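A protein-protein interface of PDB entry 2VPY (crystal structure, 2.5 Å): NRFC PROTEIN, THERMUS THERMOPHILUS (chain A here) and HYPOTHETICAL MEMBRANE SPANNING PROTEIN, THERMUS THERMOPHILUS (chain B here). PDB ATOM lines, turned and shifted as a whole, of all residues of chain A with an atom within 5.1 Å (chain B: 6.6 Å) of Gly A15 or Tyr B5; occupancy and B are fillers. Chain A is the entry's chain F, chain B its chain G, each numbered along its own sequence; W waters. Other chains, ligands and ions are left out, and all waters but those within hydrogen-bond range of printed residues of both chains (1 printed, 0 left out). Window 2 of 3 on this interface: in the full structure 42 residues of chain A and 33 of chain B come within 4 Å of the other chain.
Hydrophobic or aromatic side chains of chain A that line the printed part of chain B: Ala A17 and Trp A37.
Printed residues of chain B that touch a printed residue of chain A: Glu B3, Phe B4, Tyr B5 and Leu B7.
Hydrophobic or aromatic side chains of chain B that line the printed part of chain A: Phe B4 and Tyr B5.
Among the printed residues, no Asp or Glu carboxylate lies within 4 Å of a Lys or Arg side-chain nitrogen of the other chain.
N of Gly A15 lies close to SG of Cys A13 (3.6 Å).
N of Ile A38 is in hydrogen-bond range of O of Tyr B5, 3.0 Å away.
N of Glu A40 lies within hydrogen-bond range of O of Glu B3, 2.8 Å away.
Water W1 bridges the side-chain hydroxyl (OH) of Tyr B5 (2.7 Å) and the side-chain carboxylate (OE1) of Glu A40 (2.9 Å).
Of the printed residues of chain B, Trp A37 touches Tyr B5 (3.6 Å) and Leu B7 (3.7 Å).
Of the printed residues of chain B, Glu A40 touches Glu B3.
Phe A53 touches none of the printed residues of chain B.
Of the printed residues of chain A, Phe B4 touches Ile A38.
Of chain A, only Gly A15 (3.2 Å), Ala A17 (3.8 Å), Trp A37 (3.6 Å) and Ile A38 (3.0 Å) come within 4 Å of Tyr B5.
Gly B6 touches none of the printed residues of chain A.
The nearest printed residue of chain B that does not touch Gly A15 is Phe B4 (7.6 Å).
Tyr B5 touches Gly A15 (CE1 to O, 3.2 Å).
Tyr B5 touches Ala A17.
Tyr B5 touches Trp A37.
CB of Trp A37 touches N of Leu B7 (3.7 Å).
Glu B3 touches Ile A38.
Ile A38 touches Phe B4 (O to CA, 3.2 Å).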
ATOM      1  N   CYS A  13     -24.300 -23.615  36.583  1.00  0.00           N
ATOM      2  CA  CYS A  13     -23.449 -23.061  35.539  1.00  0.00           C
ATOM      3  C   CYS A  13     -24.328 -22.637  34.350  1.00  0.00           C
ATOM      4  O   CYS A  13     -25.183 -23.398  33.883  1.00  0.00           O
ATOM      5  CB  CYS A  13     -22.398 -24.081  35.062  1.00  0.00           C
ATOM      6  SG  CYS A  13     -20.972 -23.311  34.200  1.00  0.00           S
ATOM      7  N   VAL A  14     -24.128 -21.400  33.909  1.00  0.00           N
ATOM      8  CA  VAL A  14     -24.832 -20.839  32.763  1.00  0.00           C
ATOM      9  C   VAL A  14     -23.803 -20.647  31.645  1.00  0.00           C
ATOM     10  O   VAL A  14     -24.135 -20.161  30.585  1.00  0.00           O
ATOM     11  CB  VAL A  14     -25.536 -19.464  33.080  1.00  0.00           C
ATOM     12  CG1 VAL A  14     -26.522 -19.636  34.201  1.00  0.00           C
ATOM     13  CG2 VAL A  14     -24.504 -18.401  33.456  1.00  0.00           C
ATOM     14  N   GLY A  15     -22.554 -21.015  31.890  1.00  0.00           N
ATOM     15  CA  GLY A  15     -21.544 -20.897  30.854  1.00  0.00           C
ATOM     16  C   GLY A  15     -21.248 -19.520  30.266  1.00  0.00           C
ATOM     17  O   GLY A  15     -20.938 -19.399  29.082  1.00  0.00           O
ATOM     18  N   CYS A  16     -21.404 -18.486  31.089  1.00  0.00           N
ATOM     19  CA  CYS A  16     -21.096 -17.064  30.800  1.00  0.00           C
ATOM     20  C   CYS A  16     -19.570 -17.297  30.827  1.00  0.00           C
ATOM     21  O   CYS A  16     -19.169 -18.150  31.580  1.00  0.00           O
ATOM     22  CB  CYS A  16     -21.477 -16.262  32.051  1.00  0.00           C
ATOM     23  SG  CYS A  16     -20.486 -16.940  33.615  1.00  0.00           S
ATOM     24  N   ALA A  17     -18.641 -16.677  30.137  1.00  0.00           N
ATOM     25  CA  ALA A  17     -17.338 -17.281  30.506  1.00  0.00           C
ATOM     26  C   ALA A  17     -16.472 -16.497  31.493  1.00  0.00           C
ATOM     27  O   ALA A  17     -15.286 -16.287  31.247  1.00  0.00           O
ATOM     28  CB  ALA A  17     -16.530 -17.636  29.267  1.00  0.00           C
ATOM     29  N   TRP A  37     -11.583 -23.312  29.610  1.00  0.00           N
ATOM     30  CA  TRP A  37     -12.498 -23.034  28.510  1.00  0.00           C
ATOM     31  C   TRP A  37     -13.887 -23.631  28.868  1.00  0.00           C
ATOM     32  O   TRP A  37     -13.981 -24.441  29.783  1.00  0.00           O
ATOM     33  CB  TRP A  37     -11.943 -23.635  27.209  1.00  0.00           C
ATOM     34  CG  TRP A  37     -11.761 -25.139  27.256  1.00  0.00           C
ATOM     35  CD1 TRP A  37     -12.669 -26.086  26.867  1.00  0.00           C
ATOM     36  CD2 TRP A  37     -10.610 -25.858  27.741  1.00  0.00           C
ATOM     37  NE1 TRP A  37     -12.156 -27.342  27.079  1.00  0.00           N
ATOM     38  CE2 TRP A  37     -10.899 -27.238  27.615  1.00  0.00           C
ATOM     39  CE3 TRP A  37      -9.365 -25.470  28.276  1.00  0.00           C
ATOM     40  CZ2 TRP A  37      -9.983 -28.247  28.005  1.00  0.00           C
ATOM     41  CZ3 TRP A  37      -8.444 -26.477  28.670  1.00  0.00           C
ATOM     42  CH2 TRP A  37      -8.768 -27.851  28.528  1.00  0.00           C
ATOM     43  N   ILE A  38     -14.948 -23.216  28.173  1.00  0.00           N
ATOM     44  CA  ILE A  38     -16.314 -23.704  28.424  1.00  0.00           C
ATOM     45  C   ILE A  38     -16.776 -24.540  27.216  1.00  0.00           C
ATOM     46  O   ILE A  38     -16.447 -24.221  26.083  1.00  0.00           O
ATOM     47  CB  ILE A  38     -17.315 -22.498  28.634  1.00  0.00           C
ATOM     48  CG1 ILE A  38     -16.717 -21.505  29.635  1.00  0.00           C
ATOM     49  CG2 ILE A  38     -18.700 -22.998  29.132  1.00  0.00           C
ATOM     50  CD1 ILE A  38     -16.213 -22.153  30.923  1.00  0.00           C
ATOM     51  N   GLU A  40     -20.291 -26.260  25.569  1.00  0.00           N
ATOM     52  CA  GLU A  40     -21.748 -26.163  25.664  1.00  0.00           C
ATOM     53  C   GLU A  40     -22.321 -27.135  24.657  1.00  0.00           C
ATOM     54  O   GLU A  40     -21.982 -27.067  23.484  1.00  0.00           O
ATOM     55  CB  GLU A  40     -22.212 -24.731  25.338  1.00  0.00           C
ATOM     56  CG  GLU A  40     -23.734 -24.556  25.164  1.00  0.00           C
ATOM     57  CD  GLU A  40     -24.212 -23.084  25.098  1.00  0.00           C
ATOM     58  OE1 GLU A  40     -23.528 -22.166  25.611  1.00  0.00           O
ATOM     59  OE2 GLU A  40     -25.300 -22.852  24.545  1.00  0.00           O
ATOM     60  N   PHE A  53     -23.677 -26.872  30.234  1.00  0.00           N
ATOM     61  CA  PHE A  53     -22.640 -25.849  30.204  1.00  0.00           C
ATOM     62  C   PHE A  53     -21.582 -26.474  31.098  1.00  0.00           C
ATOM     63  O   PHE A  53     -21.829 -26.748  32.274  1.00  0.00           O
ATOM     64  CB  PHE A  53     -23.106 -24.533  30.807  1.00  0.00           C
ATOM     65  CG  PHE A  53     -24.345 -23.986  30.184  1.00  0.00           C
ATOM     66  CD1 PHE A  53     -25.601 -24.311  30.702  1.00  0.00           C
ATOM     67  CD2 PHE A  53     -24.265 -23.169  29.059  1.00  0.00           C
ATOM     68  CE1 PHE A  53     -26.762 -23.819  30.115  1.00  0.00           C
ATOM     69  CE2 PHE A  53     -25.413 -22.668  28.457  1.00  0.00           C
ATOM     70  CZ  PHE A  53     -26.668 -22.995  28.982  1.00  0.00           C
ATOM     71  N   GLU B   3     -20.122 -26.544  21.148  1.00  0.00           N
ATOM     72  CA  GLU B   3     -19.770 -25.123  20.956  1.00  0.00           C
ATOM     73  C   GLU B   3     -18.854 -24.751  22.151  1.00  0.00           C
ATOM     74  O   GLU B   3     -19.015 -25.302  23.241  1.00  0.00           O
ATOM     75  CB  GLU B   3     -21.012 -24.229  20.915  1.00  0.00           C
ATOM     76  CG  GLU B   3     -22.028 -24.669  19.870  1.00  0.00           C
ATOM     77  CD  GLU B   3     -21.897 -23.940  18.537  1.00  0.00           C
ATOM     78  OE1 GLU B   3     -21.367 -22.798  18.518  1.00  0.00           O
ATOM     79  OE2 GLU B   3     -22.346 -24.502  17.507  1.00  0.00           O
ATOM     80  N   PHE B   4     -17.889 -23.851  21.958  1.00  0.00           N
ATOM     81  CA  PHE B   4     -16.975 -23.465  23.048  1.00  0.00           C
ATOM     82  C   PHE B   4     -16.852 -21.967  23.270  1.00  0.00           C
ATOM     83  O   PHE B   4     -17.219 -21.204  22.394  1.00  0.00           O
ATOM     84  CB  PHE B   4     -15.529 -23.923  22.740  1.00  0.00           C
ATOM     85  CG  PHE B   4     -15.376 -25.377  22.520  1.00  0.00           C
ATOM     86  CD1 PHE B   4     -15.495 -25.924  21.237  1.00  0.00           C
ATOM     87  CD2 PHE B   4     -15.209 -26.225  23.601  1.00  0.00           C
ATOM     88  CE1 PHE B   4     -15.456 -27.294  21.049  1.00  0.00           C
ATOM     89  CE2 PHE B   4     -15.167 -27.592  23.425  1.00  0.00           C
ATOM     90  CZ  PHE B   4     -15.297 -28.134  22.150  1.00  0.00           C
ATOM     91  N   TYR B   5     -16.387 -21.566  24.459  1.00  0.00           N
ATOM     92  CA  TYR B   5     -15.983 -20.169  24.704  1.00  0.00           C
ATOM     93  C   TYR B   5     -14.546 -20.504  25.024  1.00  0.00           C
ATOM     94  O   TYR B   5     -14.272 -21.179  26.026  1.00  0.00           O
ATOM     95  CB  TYR B   5     -16.605 -19.500  25.900  1.00  0.00           C
ATOM     96  CG  TYR B   5     -17.980 -19.068  25.589  1.00  0.00           C
ATOM     97  CD1 TYR B   5     -19.050 -19.624  26.269  1.00  0.00           C
ATOM     98  CD2 TYR B   5     -18.230 -18.168  24.551  1.00  0.00           C
ATOM     99  CE1 TYR B   5     -20.332 -19.311  25.933  1.00  0.00           C
ATOM    100  CE2 TYR B   5     -19.522 -17.842  24.199  1.00  0.00           C
ATOM    101  CZ  TYR B   5     -20.568 -18.423  24.895  1.00  0.00           C
ATOM    102  OH  TYR B   5     -21.866 -18.143  24.541  1.00  0.00           O
ATOM    103  N   GLY B   6     -13.636 -20.054  24.163  1.00  0.00           N
ATOM    104  CA  GLY B   6     -12.233 -20.395  24.313  1.00  0.00           C
ATOM    105  C   GLY B   6     -12.077 -21.707  23.542  1.00  0.00           C
ATOM    106  O   GLY B   6     -12.902 -22.020  22.671  1.00  0.00           O
ATOM    107  N   LEU B   7     -11.055 -22.496  23.830  1.00  0.00           N
ATOM    108  CA  LEU B   7     -10.918 -23.758  23.121  1.00  0.00           C
ATOM    109  C   LEU B   7     -10.058 -24.736  23.862  1.00  0.00           C
ATOM    110  O   LEU B   7      -9.137 -24.329  24.581  1.00  0.00           O
ATOM    111  CB  LEU B   7     -10.234 -23.582  21.772  1.00  0.00           C
ATOM    112  CG  LEU B   7     -10.748 -22.809  20.568  1.00  0.00           C
ATOM    113  CD1 LEU B   7      -9.610 -22.749  19.578  1.00  0.00           C
ATOM    114  CD2 LEU B   7     -11.968 -23.493  19.936  1.00  0.00           C
HETATM  115  O   HOH W   1     -23.903 -19.292  25.870  1.00  0.00           O
